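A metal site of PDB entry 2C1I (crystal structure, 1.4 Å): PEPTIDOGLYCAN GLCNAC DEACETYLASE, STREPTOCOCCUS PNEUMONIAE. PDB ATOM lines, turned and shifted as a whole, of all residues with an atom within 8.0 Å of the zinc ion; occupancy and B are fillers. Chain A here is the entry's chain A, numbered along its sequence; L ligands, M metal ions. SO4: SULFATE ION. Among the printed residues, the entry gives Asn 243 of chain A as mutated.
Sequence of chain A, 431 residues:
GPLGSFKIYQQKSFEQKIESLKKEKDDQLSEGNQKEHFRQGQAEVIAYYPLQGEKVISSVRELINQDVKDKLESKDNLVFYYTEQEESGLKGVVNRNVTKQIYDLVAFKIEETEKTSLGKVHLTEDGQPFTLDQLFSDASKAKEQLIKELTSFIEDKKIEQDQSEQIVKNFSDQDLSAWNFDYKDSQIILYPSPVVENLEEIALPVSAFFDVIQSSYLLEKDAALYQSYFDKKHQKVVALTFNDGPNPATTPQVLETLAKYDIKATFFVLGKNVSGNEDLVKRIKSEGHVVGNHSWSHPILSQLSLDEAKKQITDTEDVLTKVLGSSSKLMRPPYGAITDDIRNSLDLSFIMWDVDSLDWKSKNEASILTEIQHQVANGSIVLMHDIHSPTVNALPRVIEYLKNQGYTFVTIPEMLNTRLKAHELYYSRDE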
ATOM      1  N   PHE A 242       3.462  -9.394   6.521  1.00  0.00           N
ATOM      2  CA  PHE A 242       2.992  -8.241   7.319  1.00  0.00           C
ATOM      3  C   PHE A 242       2.405  -7.210   6.397  1.00  0.00           C
ATOM      4  O   PHE A 242       3.113  -6.741   5.492  1.00  0.00           O
ATOM      5  CB  PHE A 242       4.169  -7.614   8.079  1.00  0.00           C
ATOM      6  CG  PHE A 242       4.751  -8.499   9.157  1.00  0.00           C
ATOM      7  CD1 PHE A 242       4.150  -8.588  10.393  1.00  0.00           C
ATOM      8  CD2 PHE A 242       5.901  -9.233   8.904  1.00  0.00           C
ATOM      9  CE1 PHE A 242       4.681  -9.427  11.360  1.00  0.00           C
ATOM     10  CE2 PHE A 242       6.418 -10.069   9.872  1.00  0.00           C
ATOM     11  CZ  PHE A 242       5.786 -10.172  11.092  1.00  0.00           C
ATOM     12  N   ASN A 243       1.142  -6.831   6.645  1.00  0.00           N
ATOM     13  CA  ASN A 243       0.484  -5.803   5.851  1.00  0.00           C
ATOM     14  C   ASN A 243       0.480  -4.428   6.511  1.00  0.00           C
ATOM     15  O   ASN A 243       0.437  -4.321   7.755  1.00  0.00           O
ATOM     16  CB  ASN A 243      -1.009  -6.164   5.700  1.00  0.00           C
ATOM     17  CG  ASN A 243      -1.263  -7.212   4.647  1.00  0.00           C
ATOM     18  OD1 ASN A 243      -0.342  -7.844   4.088  1.00  0.00           O
ATOM     19  ND2 ASN A 243      -2.551  -7.401   4.321  1.00  0.00           N
ATOM     20  N   ASP A 244       0.449  -3.398   5.665  1.00  0.00           N
ATOM     21  CA  ASP A 244      -0.024  -2.047   5.999  1.00  0.00           C
ATOM     22  C   ASP A 244       1.070  -1.089   6.409  1.00  0.00           C
ATOM     23  O   ASP A 244       0.789   0.107   6.642  1.00  0.00           O
ATOM     24  CB  ASP A 244      -1.200  -1.969   6.990  1.00  0.00           C
ATOM     25  CG  ASP A 244      -2.424  -2.704   6.536  1.00  0.00           C
ATOM     26  OD1 ASP A 244      -2.629  -2.980   5.353  1.00  0.00           O
ATOM     27  OD2 ASP A 244      -3.236  -3.040   7.433  1.00  0.00           O
ATOM     28  N   GLY A 245       2.322  -1.543   6.453  1.00  0.00           N
ATOM     29  CA  GLY A 245       3.402  -0.652   6.831  1.00  0.00           C
ATOM     30  C   GLY A 245       3.940   0.140   5.661  1.00  0.00           C
ATOM     31  O   GLY A 245       3.299   0.279   4.628  1.00  0.00           O
ATOM     32  N   PHE A 268       4.063  -6.364   2.890  1.00  0.00           N
ATOM     33  CA  PHE A 268       3.217  -5.765   1.847  1.00  0.00           C
ATOM     34  C   PHE A 268       2.878  -4.365   2.304  1.00  0.00           C
ATOM     35  O   PHE A 268       2.043  -4.155   3.201  1.00  0.00           O
ATOM     36  CB  PHE A 268       1.964  -6.629   1.620  1.00  0.00           C
ATOM     37  CG  PHE A 268       2.297  -7.934   0.921  1.00  0.00           C
ATOM     38  CD1 PHE A 268       2.457  -7.954  -0.476  1.00  0.00           C
ATOM     39  CD2 PHE A 268       2.524  -9.098   1.652  1.00  0.00           C
ATOM     40  CE1 PHE A 268       2.813  -9.142  -1.140  1.00  0.00           C
ATOM     41  CE2 PHE A 268       2.864 -10.264   0.996  1.00  0.00           C
ATOM     42  CZ  PHE A 268       3.007 -10.292  -0.387  1.00  0.00           C
ATOM     43  N   VAL A 269       3.565  -3.397   1.702  1.00  0.00           N
ATOM     44  CA  VAL A 269       3.521  -2.036   2.184  1.00  0.00           C
ATOM     45  C   VAL A 269       2.579  -1.164   1.360  1.00  0.00           C
ATOM     46  O   VAL A 269       2.329  -1.410   0.173  1.00  0.00           O
ATOM     47  CB  VAL A 269       4.934  -1.380   2.272  1.00  0.00           C
ATOM     48  CG1 VAL A 269       5.824  -2.186   3.206  1.00  0.00           C
ATOM     49  CG2 VAL A 269       5.564  -1.239   0.905  1.00  0.00           C
ATOM     50  N   LEU A 270       2.049  -0.124   2.004  1.00  0.00           N
ATOM     51  CA  LEU A 270       1.218   0.861   1.313  1.00  0.00           C
ATOM     52  C   LEU A 270       2.047   1.964   0.718  1.00  0.00           C
ATOM     53  O   LEU A 270       2.898   2.548   1.378  1.00  0.00           O
ATOM     54  CB  LEU A 270       0.221   1.485   2.318  1.00  0.00           C
ATOM     55  CG  LEU A 270      -0.938   0.551   2.696  1.00  0.00           C
ATOM     56  CD1 LEU A 270      -1.638   1.050   3.991  1.00  0.00           C
ATOM     57  CD2 LEU A 270      -1.921   0.457   1.560  1.00  0.00           C
ATOM     58  N   HIS A 294       0.994  -3.263  -1.537  1.00  0.00           N
ATOM     59  CA  HIS A 294      -0.315  -3.436  -0.892  1.00  0.00           C
ATOM     60  C   HIS A 294      -1.302  -2.342  -1.328  1.00  0.00           C
ATOM     61  O   HIS A 294      -2.237  -2.084  -0.577  1.00  0.00           O
ATOM     62  CB  HIS A 294      -0.156  -3.415   0.631  1.00  0.00           C
ATOM     63  CG  HIS A 294      -1.328  -3.928   1.399  1.00  0.00           C
ATOM     64  ND1 HIS A 294      -2.088  -5.023   1.011  1.00  0.00           N
ATOM     65  CD2 HIS A 294      -1.872  -3.505   2.577  1.00  0.00           C
ATOM     66  CE1 HIS A 294      -3.029  -5.243   1.921  1.00  0.00           C
ATOM     67  NE2 HIS A 294      -2.925  -4.333   2.875  1.00  0.00           N
ATOM     68  N   SER A 295      -1.071  -1.754  -2.516  1.00  0.00           N
ATOM     69  CA  SER A 295      -1.826  -0.608  -3.042  1.00  0.00           C
ATOM     70  C   SER A 295      -1.263   0.681  -2.494  1.00  0.00           C
ATOM     71  O   SER A 295      -0.386   0.687  -1.617  1.00  0.00           O
ATOM     72  CB  SER A 295      -3.320  -0.671  -2.844  1.00  0.00           C
ATOM     73  OG  SER A 295      -3.729  -0.229  -1.553  1.00  0.00           O
ATOM     74  N   HIS A 298      -4.966   1.768   0.232  1.00  0.00           N
ATOM     75  CA  HIS A 298      -5.812   0.758   0.882  1.00  0.00           C
ATOM     76  C   HIS A 298      -7.318   0.819   0.519  1.00  0.00           C
ATOM     77  O   HIS A 298      -8.139   0.478   1.339  1.00  0.00           O
ATOM     78  CB  HIS A 298      -5.654   0.811   2.414  1.00  0.00           C
ATOM     79  CG  HIS A 298      -5.735  -0.524   3.066  1.00  0.00           C
ATOM     80  ND1 HIS A 298      -6.913  -1.119   3.462  1.00  0.00           N
ATOM     81  CD2 HIS A 298      -4.760  -1.417   3.393  1.00  0.00           C
ATOM     82  CE1 HIS A 298      -6.665  -2.309   4.008  1.00  0.00           C
ATOM     83  NE2 HIS A 298      -5.342  -2.507   3.988  1.00  0.00           N
ATOM     84  N   PRO A 299      -7.690   1.131  -0.738  1.00  0.00           N
ATOM     85  CA  PRO A 299      -9.110   1.041  -1.094  1.00  0.00           C
ATOM     86  C   PRO A 299      -9.487  -0.423  -1.326  1.00  0.00           C
ATOM     87  O   PRO A 299      -8.602  -1.306  -1.438  1.00  0.00           O
ATOM     88  CB  PRO A 299      -9.139   1.820  -2.420  1.00  0.00           C
ATOM     89  CG  PRO A 299      -7.844   1.445  -3.058  1.00  0.00           C
ATOM     90  CD  PRO A 299      -6.834   1.452  -1.912  1.00  0.00           C
ATOM     91  N   ARG A 332      -0.365  -7.752  -2.874  1.00  0.00           N
ATOM     92  CA  ARG A 332      -1.454  -8.284  -2.065  1.00  0.00           C
ATOM     93  C   ARG A 332      -2.612  -7.283  -2.024  1.00  0.00           C
ATOM     94  O   ARG A 332      -2.462  -6.189  -1.457  1.00  0.00           O
ATOM     95  CB  ARG A 332      -1.014  -8.589  -0.616  1.00  0.00           C
ATOM     96  CG  ARG A 332      -2.204  -9.052   0.226  1.00  0.00           C
ATOM     97  CD  ARG A 332      -1.733  -9.562   1.579  1.00  0.00           C
ATOM     98  NE  ARG A 332      -1.047 -10.835   1.468  1.00  0.00           N
ATOM     99  CZ  ARG A 332      -0.320 -11.336   2.468  1.00  0.00           C
ATOM    100  NH1 ARG A 332      -0.046 -10.600   3.568  1.00  0.00           N
ATOM    101  NH2 ARG A 332       0.185 -12.543   2.368  1.00  0.00           N
ATOM    102  N   PRO A 333      -3.752  -7.619  -2.621  1.00  0.00           N
ATOM    103  CA  PRO A 333      -4.931  -6.728  -2.543  1.00  0.00           C
ATOM    104  C   PRO A 333      -5.452  -6.494  -1.135  1.00  0.00           C
ATOM    105  O   PRO A 333      -5.721  -7.468  -0.421  1.00  0.00           O
ATOM    106  CB  PRO A 333      -5.962  -7.449  -3.415  1.00  0.00           C
ATOM    107  CG  PRO A 333      -5.104  -8.301  -4.396  1.00  0.00           C
ATOM    108  CD  PRO A 333      -4.000  -8.790  -3.496  1.00  0.00           C
ATOM    109  N   PRO A 334      -5.673  -5.226  -0.743  1.00  0.00           N
ATOM    110  CA  PRO A 334      -6.424  -4.939   0.506  1.00  0.00           C
ATOM    111  C   PRO A 334      -7.712  -5.739   0.558  1.00  0.00           C
ATOM    112  O   PRO A 334      -8.454  -5.827  -0.443  1.00  0.00           O
ATOM    113  CB  PRO A 334      -6.673  -3.416   0.430  1.00  0.00           C
ATOM    114  CG  PRO A 334      -5.507  -2.929  -0.410  1.00  0.00           C
ATOM    115  CD  PRO A 334      -5.262  -4.005  -1.437  1.00  0.00           C
ATOM    116  N   TYR A 335      -7.965  -6.331   1.710  1.00  0.00           N
ATOM    117  CA  TYR A 335      -9.202  -7.071   1.971  1.00  0.00           C
ATOM    118  C   TYR A 335      -9.304  -8.343   1.126  1.00  0.00           C
ATOM    119  O   TYR A 335     -10.323  -9.023   1.170  1.00  0.00           O
ATOM    120  CB  TYR A 335     -10.485  -6.175   1.780  1.00  0.00           C
ATOM    121  CG  TYR A 335     -10.345  -4.805   2.382  1.00  0.00           C
ATOM    122  CD1 TYR A 335     -10.439  -4.634   3.765  1.00  0.00           C
ATOM    123  CD2 TYR A 335     -10.091  -3.681   1.591  1.00  0.00           C
ATOM    124  CE1 TYR A 335     -10.288  -3.388   4.340  1.00  0.00           C
ATOM    125  CE2 TYR A 335      -9.947  -2.434   2.173  1.00  0.00           C
ATOM    126  CZ  TYR A 335     -10.038  -2.283   3.534  1.00  0.00           C
ATOM    127  OH  TYR A 335      -9.816  -1.039   4.094  1.00  0.00           O
ATOM    128  N   GLY A 336      -8.245  -8.665   0.363  1.00  0.00           N
ATOM    129  CA  GLY A 336      -8.343  -9.803  -0.553  1.00  0.00           C
ATOM    130  C   GLY A 336      -9.230  -9.514  -1.761  1.00  0.00           C
ATOM    131  O   GLY A 336      -9.593 -10.434  -2.517  1.00  0.00           O
ATOM    132  N   TRP A 353      -3.388 -15.364   1.270  1.00  0.00           N
ATOM    133  CA  TRP A 353      -2.892 -16.035   2.488  1.00  0.00           C
ATOM    134  C   TRP A 353      -3.841 -17.180   2.776  1.00  0.00           C
ATOM    135  O   TRP A 353      -4.928 -17.212   2.217  1.00  0.00           O
ATOM    136  CB  TRP A 353      -2.860 -15.063   3.686  1.00  0.00           C
ATOM    137  CG  TRP A 353      -4.222 -14.496   4.022  1.00  0.00           C
ATOM    138  CD1 TRP A 353      -5.133 -15.007   4.932  1.00  0.00           C
ATOM    139  CD2 TRP A 353      -4.812 -13.320   3.469  1.00  0.00           C
ATOM    140  NE1 TRP A 353      -6.266 -14.213   4.954  1.00  0.00           N
ATOM    141  CE2 TRP A 353      -6.089 -13.182   4.073  1.00  0.00           C
ATOM    142  CE3 TRP A 353      -4.393 -12.374   2.527  1.00  0.00           C
ATOM    143  CZ2 TRP A 353      -6.937 -12.121   3.762  1.00  0.00           C
ATOM    144  CZ3 TRP A 353      -5.217 -11.308   2.223  1.00  0.00           C
ATOM    145  CH2 TRP A 353      -6.502 -11.208   2.811  1.00  0.00           C
ATOM    146  N   LEU A 383      -0.950 -14.207   7.643  1.00  0.00           N
ATOM    147  CA  LEU A 383      -1.240 -12.780   7.612  1.00  0.00           C
ATOM    148  C   LEU A 383      -1.135 -12.150   9.011  1.00  0.00           C
ATOM    149  O   LEU A 383      -1.830 -12.592   9.938  1.00  0.00           O
ATOM    150  CB  LEU A 383      -2.658 -12.553   7.046  1.00  0.00           C
ATOM    151  CG  LEU A 383      -3.149 -11.092   7.095  1.00  0.00           C
ATOM    152  CD1 LEU A 383      -2.303 -10.182   6.221  1.00  0.00           C
ATOM    153  CD2 LEU A 383      -4.634 -11.033   6.683  1.00  0.00           C
ATOM    154  N   MET A 384      -0.278 -11.130   9.127  1.00  0.00           N
ATOM    155  CA  MET A 384      -0.210 -10.235  10.286  1.00  0.00           C
ATOM    156  C   MET A 384      -0.178  -8.828   9.800  1.00  0.00           C
ATOM    157  O   MET A 384       0.001  -8.576   8.595  1.00  0.00           O
ATOM    158  CB  MET A 384       1.029 -10.541  11.096  1.00  0.00           C
ATOM    159  CG  MET A 384       0.971 -11.944  11.794  1.00  0.00           C
ATOM    160  SD  MET A 384       2.404 -12.268  12.794  1.00  0.00           S
ATOM    161  CE  MET A 384       1.982 -13.806  13.550  1.00  0.00           C
ATOM    162  N   HIS A 385      -0.293  -7.894  10.734  1.00  0.00           N
ATOM    163  CA  HIS A 385      -0.276  -6.432  10.422  1.00  0.00           C
ATOM    164  C   HIS A 385       0.755  -5.826  11.351  1.00  0.00           C
ATOM    165  O   HIS A 385       0.514  -5.842  12.561  1.00  0.00           O
ATOM    166  CB  HIS A 385      -1.685  -5.840  10.654  1.00  0.00           C
ATOM    167  CG  HIS A 385      -2.757  -6.473   9.815  1.00  0.00           C
ATOM    168  ND1 HIS A 385      -3.317  -7.695  10.113  1.00  0.00           N
ATOM    169  CD2 HIS A 385      -3.334  -6.075   8.654  1.00  0.00           C
ATOM    170  CE1 HIS A 385      -4.190  -8.046   9.176  1.00  0.00           C
ATOM    171  NE2 HIS A 385      -4.231  -7.062   8.286  1.00  0.00           N
ATOM    172  N   ILE A 387       1.541  -3.028  12.452  1.00  0.00           N
ATOM    173  CA  ILE A 387       1.211  -1.640  12.710  1.00  0.00           C
ATOM    174  C   ILE A 387       0.690  -1.406  14.118  1.00  0.00           C
ATOM    175  O   ILE A 387       0.520  -0.239  14.491  1.00  0.00           O
ATOM    176  CB  ILE A 387       0.354  -1.011  11.526  1.00  0.00           C
ATOM    177  CG1 ILE A 387      -0.910  -1.818  11.224  1.00  0.00           C
ATOM    178  CG2 ILE A 387       1.216  -0.910  10.234  1.00  0.00           C
ATOM    179  CD1 ILE A 387      -0.652  -2.940  10.244  1.00  0.00           C
HETATM  180  S   SO4 L   1      -6.014  -6.155   5.242  1.00  0.00           S
HETATM  181  O1  SO4 L   1      -7.013  -5.024   5.544  1.00  0.00           O
HETATM  182  O2  SO4 L   1      -6.379  -6.644   3.865  1.00  0.00           O
HETATM  183  O3  SO4 L   1      -4.619  -5.627   5.317  1.00  0.00           O
HETATM  184  O4  SO4 L   1      -6.105  -7.164   6.344  1.00  0.00           O
HETATM  185 ZN    ZN M   1      -4.055  -3.952   4.526  1.00  0.00          ZN
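N of His 294 lies within hydrogen-bond range of O of Val 269, 2.9 Å away. N of Asp 244 sits at hydrogen-bond distance from O of Phe 268 (3.0 Å). A ring nitrogen (NE2) of His 294 lies close to the side-chain amide nitrogen (ND2) of Asn 243 (3.4 Å). A ring nitrogen (ND1) of His 298 sits at hydrogen-bond distance from the side-chain hydroxyl of Tyr 335, at 3.0 Å. N of Asn 243 sits at hydrogen-bond distance from O of Met 384 (2.9 Å). A ring nitrogen (ND1) of His 294 sits at hydrogen-bond distance from the backbone carbonyl oxygen (O) of Arg 332. The side-chain amide oxygen of Asn 243 lies within hydrogen-bond range of the guanidinium group of Arg 332 (2.8 Å). N of His 298 lies within hydrogen-bond range of OG of Ser 295, at 3.0 Å.
The zinc ion is bound by OD1 of Asp 244 (1.9 Å), O3 of the ligand (1.9 Å), NE2 of His 298 (2.0 Å) and NE2 of His 294 (2.0 Å). The zinc ion has four donor atoms within binding distance.
Asn 243 touches the zinc ion (ND2 to ZN, 3.8 Å). Four residues have an atom within 4 Å of the zinc ion: Asn 243, Asp 244, His 294 and His 298. The nearest printed residue that does not touch the zinc ion is His 385 (4.7 Å).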
